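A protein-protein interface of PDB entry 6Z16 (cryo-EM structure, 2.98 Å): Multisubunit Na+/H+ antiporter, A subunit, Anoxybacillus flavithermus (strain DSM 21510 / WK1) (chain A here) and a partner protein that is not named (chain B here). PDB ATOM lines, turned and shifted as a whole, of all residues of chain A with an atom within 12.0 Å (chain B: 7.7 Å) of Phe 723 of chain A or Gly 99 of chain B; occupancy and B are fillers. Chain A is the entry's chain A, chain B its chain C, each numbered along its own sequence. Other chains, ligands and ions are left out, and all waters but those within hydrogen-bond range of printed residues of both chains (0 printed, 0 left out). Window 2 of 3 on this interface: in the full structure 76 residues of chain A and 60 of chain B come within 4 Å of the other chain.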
ATOM      1  N   ARG A 672     -20.177 -25.623 -35.342  1.00  0.00           N
ATOM      2  CA  ARG A 672     -21.213 -24.695 -35.774  1.00  0.00           C
ATOM      3  C   ARG A 672     -20.713 -23.265 -35.921  1.00  0.00           C
ATOM      4  O   ARG A 672     -21.269 -22.515 -36.734  1.00  0.00           O
ATOM      5  CB  ARG A 672     -22.390 -24.757 -34.800  1.00  0.00           C
ATOM      6  CG  ARG A 672     -23.216 -26.015 -34.975  1.00  0.00           C
ATOM      7  CD  ARG A 672     -24.413 -26.067 -34.061  1.00  0.00           C
ATOM      8  NE  ARG A 672     -24.017 -26.300 -32.678  1.00  0.00           N
ATOM      9  CZ  ARG A 672     -23.892 -27.504 -32.135  1.00  0.00           C
ATOM     10  NH1 ARG A 672     -24.138 -28.582 -32.858  1.00  0.00           N
ATOM     11  NH2 ARG A 672     -23.528 -27.630 -30.867  1.00  0.00           N
ATOM     12  N   CYS A 716     -27.067 -16.700 -30.599  1.00  0.00           N
ATOM     13  CA  CYS A 716     -27.760 -17.981 -30.525  1.00  0.00           C
ATOM     14  C   CYS A 716     -26.815 -19.153 -30.261  1.00  0.00           C
ATOM     15  O   CYS A 716     -27.253 -20.168 -29.711  1.00  0.00           O
ATOM     16  CB  CYS A 716     -28.549 -18.199 -31.814  1.00  0.00           C
ATOM     17  SG  CYS A 716     -29.658 -19.605 -31.820  1.00  0.00           S
ATOM     18  N   PHE A 717     -25.531 -19.034 -30.618  1.00  0.00           N
ATOM     19  CA  PHE A 717     -24.590 -20.137 -30.428  1.00  0.00           C
ATOM     20  C   PHE A 717     -24.237 -20.330 -28.958  1.00  0.00           C
ATOM     21  O   PHE A 717     -24.430 -21.414 -28.401  1.00  0.00           O
ATOM     22  CB  PHE A 717     -23.312 -19.907 -31.241  1.00  0.00           C
ATOM     23  CG  PHE A 717     -22.282 -20.994 -31.063  1.00  0.00           C
ATOM     24  CD1 PHE A 717     -22.410 -22.200 -31.727  1.00  0.00           C
ATOM     25  CD2 PHE A 717     -21.198 -20.820 -30.209  1.00  0.00           C
ATOM     26  CE1 PHE A 717     -21.471 -23.206 -31.554  1.00  0.00           C
ATOM     27  CE2 PHE A 717     -20.268 -21.825 -30.023  1.00  0.00           C
ATOM     28  CZ  PHE A 717     -20.403 -23.016 -30.700  1.00  0.00           C
ATOM     29  N   TYR A 718     -23.697 -19.294 -28.313  1.00  0.00           N
ATOM     30  CA  TYR A 718     -23.071 -19.436 -26.999  1.00  0.00           C
ATOM     31  C   TYR A 718     -24.046 -19.707 -25.864  1.00  0.00           C
ATOM     32  O   TYR A 718     -23.596 -19.818 -24.720  1.00  0.00           O
ATOM     33  CB  TYR A 718     -22.255 -18.189 -26.659  1.00  0.00           C
ATOM     34  CG  TYR A 718     -20.959 -18.064 -27.423  1.00  0.00           C
ATOM     35  CD1 TYR A 718     -19.844 -18.796 -27.047  1.00  0.00           C
ATOM     36  CD2 TYR A 718     -20.844 -17.201 -28.505  1.00  0.00           C
ATOM     37  CE1 TYR A 718     -18.657 -18.690 -27.734  1.00  0.00           C
ATOM     38  CE2 TYR A 718     -19.657 -17.084 -29.198  1.00  0.00           C
ATOM     39  CZ  TYR A 718     -18.567 -17.833 -28.806  1.00  0.00           C
ATOM     40  OH  TYR A 718     -17.379 -17.724 -29.490  1.00  0.00           O
ATOM     41  N   HIS A 719     -25.348 -19.810 -26.124  1.00  0.00           N
ATOM     42  CA  HIS A 719     -26.310 -20.227 -25.113  1.00  0.00           C
ATOM     43  C   HIS A 719     -26.898 -21.600 -25.408  1.00  0.00           C
ATOM     44  O   HIS A 719     -27.984 -21.918 -24.915  1.00  0.00           O
ATOM     45  CB  HIS A 719     -27.423 -19.192 -24.976  1.00  0.00           C
ATOM     46  CG  HIS A 719     -26.954 -17.884 -24.424  1.00  0.00           C
ATOM     47  ND1 HIS A 719     -26.494 -16.863 -25.224  1.00  0.00           N
ATOM     48  CD2 HIS A 719     -26.856 -17.439 -23.150  1.00  0.00           C
ATOM     49  CE1 HIS A 719     -26.142 -15.840 -24.468  1.00  0.00           C
ATOM     50  NE2 HIS A 719     -26.350 -16.163 -23.205  1.00  0.00           N
ATOM     51  N   LEU A 720     -26.215 -22.405 -26.218  1.00  0.00           N
ATOM     52  CA  LEU A 720     -26.581 -23.806 -26.356  1.00  0.00           C
ATOM     53  C   LEU A 720     -26.365 -24.524 -25.028  1.00  0.00           C
ATOM     54  O   LEU A 720     -25.419 -24.202 -24.299  1.00  0.00           O
ATOM     55  CB  LEU A 720     -25.756 -24.479 -27.453  1.00  0.00           C
ATOM     56  CG  LEU A 720     -26.157 -24.184 -28.893  1.00  0.00           C
ATOM     57  CD1 LEU A 720     -25.123 -24.703 -29.856  1.00  0.00           C
ATOM     58  CD2 LEU A 720     -27.479 -24.836 -29.163  1.00  0.00           C
ATOM     59  N   PRO A 721     -27.231 -25.476 -24.670  1.00  0.00           N
ATOM     60  CA  PRO A 721     -27.058 -26.188 -23.397  1.00  0.00           C
ATOM     61  C   PRO A 721     -25.842 -27.101 -23.419  1.00  0.00           C
ATOM     62  O   PRO A 721     -25.560 -27.767 -24.415  1.00  0.00           O
ATOM     63  CB  PRO A 721     -28.357 -26.987 -23.261  1.00  0.00           C
ATOM     64  CG  PRO A 721     -28.859 -27.129 -24.652  1.00  0.00           C
ATOM     65  CD  PRO A 721     -28.466 -25.877 -25.365  1.00  0.00           C
ATOM     66  N   LYS A 722     -25.116 -27.117 -22.299  1.00  0.00           N
ATOM     67  CA  LYS A 722     -23.831 -27.805 -22.255  1.00  0.00           C
ATOM     68  C   LYS A 722     -23.993 -29.319 -22.243  1.00  0.00           C
ATOM     69  O   LYS A 722     -23.098 -30.036 -22.704  1.00  0.00           O
ATOM     70  CB  LYS A 722     -23.031 -27.341 -21.040  1.00  0.00           C
ATOM     71  CG  LYS A 722     -22.575 -25.893 -21.124  1.00  0.00           C
ATOM     72  CD  LYS A 722     -21.762 -25.493 -19.906  1.00  0.00           C
ATOM     73  CE  LYS A 722     -21.328 -24.037 -19.983  1.00  0.00           C
ATOM     74  NZ  LYS A 722     -20.541 -23.626 -18.788  1.00  0.00           N
ATOM     75  N   PHE A 723     -25.103 -29.823 -21.716  1.00  0.00           N
ATOM     76  CA  PHE A 723     -25.400 -31.239 -21.867  1.00  0.00           C
ATOM     77  C   PHE A 723     -25.943 -31.496 -23.267  1.00  0.00           C
ATOM     78  O   PHE A 723     -26.405 -30.574 -23.945  1.00  0.00           O
ATOM     79  CB  PHE A 723     -26.384 -31.714 -20.791  1.00  0.00           C
ATOM     80  CG  PHE A 723     -27.763 -31.106 -20.886  1.00  0.00           C
ATOM     81  CD1 PHE A 723     -28.035 -29.875 -20.305  1.00  0.00           C
ATOM     82  CD2 PHE A 723     -28.801 -31.797 -21.496  1.00  0.00           C
ATOM     83  CE1 PHE A 723     -29.300 -29.323 -20.375  1.00  0.00           C
ATOM     84  CE2 PHE A 723     -30.069 -31.249 -21.566  1.00  0.00           C
ATOM     85  CZ  PHE A 723     -30.318 -30.012 -21.002  1.00  0.00           C
ATOM     86  N   THR A 724     -25.786 -32.752 -23.721  1.00  0.00           N
ATOM     87  CA  THR A 724     -26.187 -33.325 -25.032  1.00  0.00           C
ATOM     88  C   THR A 724     -25.727 -32.487 -26.243  1.00  0.00           C
ATOM     89  O   THR A 724     -26.209 -32.680 -27.366  1.00  0.00           O
ATOM     90  CB  THR A 724     -27.702 -33.647 -25.106  1.00  0.00           C
ATOM     91  OG1 THR A 724     -27.945 -34.513 -26.220  1.00  0.00           O
ATOM     92  CG2 THR A 724     -28.633 -32.420 -25.257  1.00  0.00           C
ATOM     93  N   GLN A 725     -24.733 -31.618 -26.061  1.00  0.00           N
ATOM     94  CA  GLN A 725     -24.269 -30.743 -27.136  1.00  0.00           C
ATOM     95  C   GLN A 725     -23.270 -31.473 -28.030  1.00  0.00           C
ATOM     96  O   GLN A 725     -23.526 -31.688 -29.219  1.00  0.00           O
ATOM     97  CB  GLN A 725     -23.675 -29.476 -26.509  1.00  0.00           C
ATOM     98  CG  GLN A 725     -23.295 -28.340 -27.442  1.00  0.00           C
ATOM     99  CD  GLN A 725     -21.891 -28.468 -27.981  1.00  0.00           C
ATOM    100  OE1 GLN A 725     -21.668 -28.387 -29.187  1.00  0.00           O
ATOM    101  NE2 GLN A 725     -20.932 -28.675 -27.087  1.00  0.00           N
ATOM    102  N   LYS A 726     -22.095 -31.796 -27.474  1.00  0.00           N
ATOM    103  CA  LYS A 726     -21.107 -32.767 -27.960  1.00  0.00           C
ATOM    104  C   LYS A 726     -20.355 -32.351 -29.229  1.00  0.00           C
ATOM    105  O   LYS A 726     -19.316 -32.947 -29.541  1.00  0.00           O
ATOM    106  CB  LYS A 726     -21.774 -34.131 -28.180  1.00  0.00           C
ATOM    107  CG  LYS A 726     -22.304 -34.774 -26.908  1.00  0.00           C
ATOM    108  CD  LYS A 726     -23.108 -36.032 -27.208  1.00  0.00           C
ATOM    109  CE  LYS A 726     -22.215 -37.182 -27.625  1.00  0.00           C
ATOM    110  NZ  LYS A 726     -21.375 -37.661 -26.497  1.00  0.00           N
ATOM    111  N   GLN A 727     -20.821 -31.292 -29.898  1.00  0.00           N
ATOM    112  CA  GLN A 727     -20.235 -30.685 -31.102  1.00  0.00           C
ATOM    113  C   GLN A 727     -19.925 -31.722 -32.192  1.00  0.00           C
ATOM    114  O   GLN A 727     -18.773 -32.017 -32.513  1.00  0.00           O
ATOM    115  CB  GLN A 727     -18.997 -29.864 -30.747  1.00  0.00           C
ATOM    116  CG  GLN A 727     -18.632 -28.857 -31.819  1.00  0.00           C
ATOM    117  CD  GLN A 727     -19.755 -27.866 -32.047  1.00  0.00           C
ATOM    118  OE1 GLN A 727     -20.480 -27.944 -33.038  1.00  0.00           O
ATOM    119  NE2 GLN A 727     -19.920 -26.940 -31.112  1.00  0.00           N
ATOM    120  N   GLU A 728     -20.987 -32.298 -32.742  1.00  0.00           N
ATOM    121  CA  GLU A 728     -20.861 -33.371 -33.714  1.00  0.00           C
ATOM    122  C   GLU A 728     -21.102 -32.836 -35.126  1.00  0.00           C
ATOM    123  O   GLU A 728     -21.793 -31.833 -35.328  1.00  0.00           O
ATOM    124  CB  GLU A 728     -21.831 -34.509 -33.360  1.00  0.00           C
ATOM    125  CG  GLU A 728     -21.529 -35.867 -33.987  1.00  0.00           C
ATOM    126  CD  GLU A 728     -22.292 -36.121 -35.269  1.00  0.00           C
ATOM    127  OE1 GLU A 728     -23.451 -35.666 -35.370  1.00  0.00           O
ATOM    128  OE2 GLU A 728     -21.730 -36.769 -36.176  1.00  0.00           O
ATOM    129  N   ARG B  93     -35.124 -18.442 -27.209  1.00  0.00           N
ATOM    130  CA  ARG B  93     -36.142 -18.690 -26.190  1.00  0.00           C
ATOM    131  C   ARG B  93     -36.399 -20.179 -26.003  1.00  0.00           C
ATOM    132  O   ARG B  93     -36.567 -20.652 -24.870  1.00  0.00           O
ATOM    133  CB  ARG B  93     -37.439 -17.976 -26.562  1.00  0.00           C
ATOM    134  CG  ARG B  93     -37.355 -16.475 -26.514  1.00  0.00           C
ATOM    135  CD  ARG B  93     -37.123 -16.067 -25.100  1.00  0.00           C
ATOM    136  NE  ARG B  93     -38.235 -16.508 -24.278  1.00  0.00           N
ATOM    137  CZ  ARG B  93     -38.157 -16.698 -22.972  1.00  0.00           C
ATOM    138  NH1 ARG B  93     -37.010 -16.499 -22.347  1.00  0.00           N
ATOM    139  NH2 ARG B  93     -39.220 -17.099 -22.297  1.00  0.00           N
ATOM    140  N   SER B  94     -36.425 -20.933 -27.104  1.00  0.00           N
ATOM    141  CA  SER B  94     -36.658 -22.368 -27.001  1.00  0.00           C
ATOM    142  C   SER B  94     -35.468 -23.095 -26.388  1.00  0.00           C
ATOM    143  O   SER B  94     -35.658 -24.106 -25.709  1.00  0.00           O
ATOM    144  CB  SER B  94     -36.978 -22.951 -28.369  1.00  0.00           C
ATOM    145  OG  SER B  94     -35.841 -22.906 -29.205  1.00  0.00           O
ATOM    146  N   TYR B  95     -34.241 -22.616 -26.623  1.00  0.00           N
ATOM    147  CA  TYR B  95     -33.093 -23.163 -25.902  1.00  0.00           C
ATOM    148  C   TYR B  95     -33.204 -22.872 -24.416  1.00  0.00           C
ATOM    149  O   TYR B  95     -32.825 -23.703 -23.583  1.00  0.00           O
ATOM    150  CB  TYR B  95     -31.776 -22.578 -26.410  1.00  0.00           C
ATOM    151  CG  TYR B  95     -31.377 -22.908 -27.825  1.00  0.00           C
ATOM    152  CD1 TYR B  95     -31.963 -23.953 -28.522  1.00  0.00           C
ATOM    153  CD2 TYR B  95     -30.410 -22.150 -28.469  1.00  0.00           C
ATOM    154  CE1 TYR B  95     -31.594 -24.233 -29.823  1.00  0.00           C
ATOM    155  CE2 TYR B  95     -30.038 -22.422 -29.762  1.00  0.00           C
ATOM    156  CZ  TYR B  95     -30.628 -23.462 -30.437  1.00  0.00           C
ATOM    157  OH  TYR B  95     -30.245 -23.730 -31.730  1.00  0.00           O
ATOM    158  N   GLN B  96     -33.711 -21.688 -24.066  1.00  0.00           N
ATOM    159  CA  GLN B  96     -33.737 -21.300 -22.660  1.00  0.00           C
ATOM    160  C   GLN B  96     -34.802 -22.063 -21.879  1.00  0.00           C
ATOM    161  O   GLN B  96     -34.558 -22.483 -20.742  1.00  0.00           O
ATOM    162  CB  GLN B  96     -33.955 -19.793 -22.538  1.00  0.00           C
ATOM    163  CG  GLN B  96     -33.788 -19.267 -21.126  1.00  0.00           C
ATOM    164  CD  GLN B  96     -33.940 -17.765 -21.047  1.00  0.00           C
ATOM    165  OE1 GLN B  96     -34.247 -17.109 -22.042  1.00  0.00           O
ATOM    166  NE2 GLN B  96     -33.717 -17.210 -19.863  1.00  0.00           N
ATOM    167  N   GLU B  97     -35.986 -22.266 -22.466  1.00  0.00           N
ATOM    168  CA  GLU B  97     -37.065 -22.861 -21.679  1.00  0.00           C
ATOM    169  C   GLU B  97     -37.193 -24.371 -21.847  1.00  0.00           C
ATOM    170  O   GLU B  97     -37.402 -25.079 -20.855  1.00  0.00           O
ATOM    171  CB  GLU B  97     -38.399 -22.188 -22.005  1.00  0.00           C
ATOM    172  CG  GLU B  97     -38.497 -20.784 -21.432  1.00  0.00           C
ATOM    173  CD  GLU B  97     -39.853 -20.153 -21.637  1.00  0.00           C
ATOM    174  OE1 GLU B  97     -40.701 -20.766 -22.318  1.00  0.00           O
ATOM    175  OE2 GLU B  97     -40.070 -19.038 -21.115  1.00  0.00           O
ATOM    176  N   ILE B  98     -37.088 -24.891 -23.070  1.00  0.00           N
ATOM    177  CA  ILE B  98     -37.159 -26.338 -23.261  1.00  0.00           C
ATOM    178  C   ILE B  98     -35.862 -26.992 -22.803  1.00  0.00           C
ATOM    179  O   ILE B  98     -35.848 -27.793 -21.861  1.00  0.00           O
ATOM    180  CB  ILE B  98     -37.472 -26.674 -24.729  1.00  0.00           C
ATOM    181  CG1 ILE B  98     -38.827 -26.092 -25.122  1.00  0.00           C
ATOM    182  CG2 ILE B  98     -37.453 -28.167 -24.948  1.00  0.00           C
ATOM    183  CD1 ILE B  98     -39.102 -26.130 -26.602  1.00  0.00           C
ATOM    184  N   GLY B  99     -34.754 -26.649 -23.450  1.00  0.00           N
ATOM    185  CA  GLY B  99     -33.459 -27.130 -23.017  1.00  0.00           C
ATOM    186  C   GLY B  99     -32.811 -28.117 -23.961  1.00  0.00           C
ATOM    187  O   GLY B  99     -32.019 -28.956 -23.524  1.00  0.00           O
ATOM    188  N   THR B 100     -33.124 -28.036 -25.253  1.00  0.00           N
ATOM    189  CA  THR B 100     -32.538 -28.957 -26.213  1.00  0.00           C
ATOM    190  C   THR B 100     -32.450 -28.294 -27.579  1.00  0.00           C
ATOM    191  O   THR B 100     -33.132 -27.308 -27.865  1.00  0.00           O
ATOM    192  CB  THR B 100     -33.334 -30.267 -26.307  1.00  0.00           C
ATOM    193  OG1 THR B 100     -32.628 -31.197 -27.136  1.00  0.00           O
ATOM    194  CG2 THR B 100     -34.716 -30.026 -26.890  1.00  0.00           C
ATOM    195  N   ASP B 101     -31.586 -28.858 -28.423  1.00  0.00           N
ATOM    196  CA  ASP B 101     -31.361 -28.372 -29.775  1.00  0.00           C
ATOM    197  C   ASP B 101     -31.821 -29.365 -30.835  1.00  0.00           C
ATOM    198  O   ASP B 101     -31.971 -28.981 -32.000  1.00  0.00           O
ATOM    199  CB  ASP B 101     -29.865 -28.076 -29.974  1.00  0.00           C
ATOM    200  CG  ASP B 101     -29.591 -27.160 -31.148  1.00  0.00           C
ATOM    201  OD1 ASP B 101     -30.538 -26.589 -31.718  1.00  0.00           O
ATOM    202  OD2 ASP B 101     -28.412 -27.040 -31.534  1.00  0.00           O
ATOM    203  N   HIS B 102     -32.065 -30.620 -30.459  1.00  0.00           N
ATOM    204  CA  HIS B 102     -32.361 -31.665 -31.429  1.00  0.00           C
ATOM    205  C   HIS B 102     -33.762 -31.476 -31.995  1.00  0.00           C
ATOM    206  O   HIS B 102     -34.749 -31.488 -31.252  1.00  0.00           O
ATOM    207  CB  HIS B 102     -32.214 -33.032 -30.771  1.00  0.00           C
ATOM    208  CG  HIS B 102     -30.815 -33.332 -30.330  1.00  0.00           C
ATOM    209  ND1 HIS B 102     -30.338 -32.988 -29.084  1.00  0.00           N
ATOM    210  CD2 HIS B 102     -29.785 -33.925 -30.977  1.00  0.00           C
ATOM    211  CE1 HIS B 102     -29.076 -33.366 -28.978  1.00  0.00           C
ATOM    212  NE2 HIS B 102     -28.717 -33.939 -30.112  1.00  0.00           N
ATOM    213  N   MET B 106     -37.727 -32.812 -30.737  1.00  0.00           N
ATOM    214  CA  MET B 106     -38.834 -31.918 -30.403  1.00  0.00           C
ATOM    215  C   MET B 106     -40.149 -32.614 -30.727  1.00  0.00           C
ATOM    216  O   MET B 106     -40.537 -32.730 -31.891  1.00  0.00           O
ATOM    217  CB  MET B 106     -38.717 -30.601 -31.161  1.00  0.00           C
ATOM    218  CG  MET B 106     -37.574 -29.711 -30.705  1.00  0.00           C
ATOM    219  SD  MET B 106     -37.559 -28.120 -31.550  1.00  0.00           S
ATOM    220  CE  MET B 106     -36.079 -27.380 -30.872  1.00  0.00           C
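Among the printed residues, merely in contact across the chains: Cys 716 of chain A with Tyr 95 of chain B (3.5 Å), Leu 720 of chain A with Tyr 95 of chain B (3.6 Å), Leu 720 of chain A with Asp 101 of chain B (3.4 Å), Pro 721 of chain A with Gly 99 of chain B (3.8 Å), Phe 723 of chain A with Gly 99 of chain B (3.2 Å) and Thr 724 of chain A with His 102 of chain B (3.2 Å).
Of the 11 printed residues of chain B, 4 touch a printed residue of chain A.
Hydrophobic or aromatic side chains of chain B within 4 Å of the printed part of chain A: Tyr 95 and His 102.
Hydrophobic or aromatic side chains of chain A within 4 Å of the printed part of chain B: Leu 720, Pro 721 and Phe 723.
Along chain A the printed residues that touch a printed residue of chain B span positions 716 to 724.
OH of Tyr 95 of chain B lies within hydrogen-bond range of OD1 of Asp 101 of chain B.
The backbone NH (N) of His 102 of chain B sits at hydrogen-bond distance from the side-chain hydroxyl (OG1) of Thr 100 of chain B (3.4 Å).
Of the printed residues of chain B, Cys 716 of chain A touches Tyr 95.
Printed residues of chain B within 4 Å of Leu 720 of chain A: Tyr 95 and Asp 101.
Printed residues of chain B within 4 Å of Pro 721 of chain A: Gly 99.
Of the printed residues of chain B, Phe 723 of chain A touches Gly 99.
Of the printed residues of chain B, Thr 724 of chain A touches His 102.
Ser 94 of chain B touches none of the printed residues of chain A.
No residue of chain A comes within 4 Å of Ile 98 of chain B.
Gly 99 of chain B touches two residues of chain A.
Thr 100 of chain B touches none of the printed residues of chain A.
Printed residues of chain A within 4 Å of His 102 of chain B: Thr 724 (3.2 Å).
The nearest residue of chain A that does not touch Gly 99 of chain B is Thr 724 of chain A (5.1 Å).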
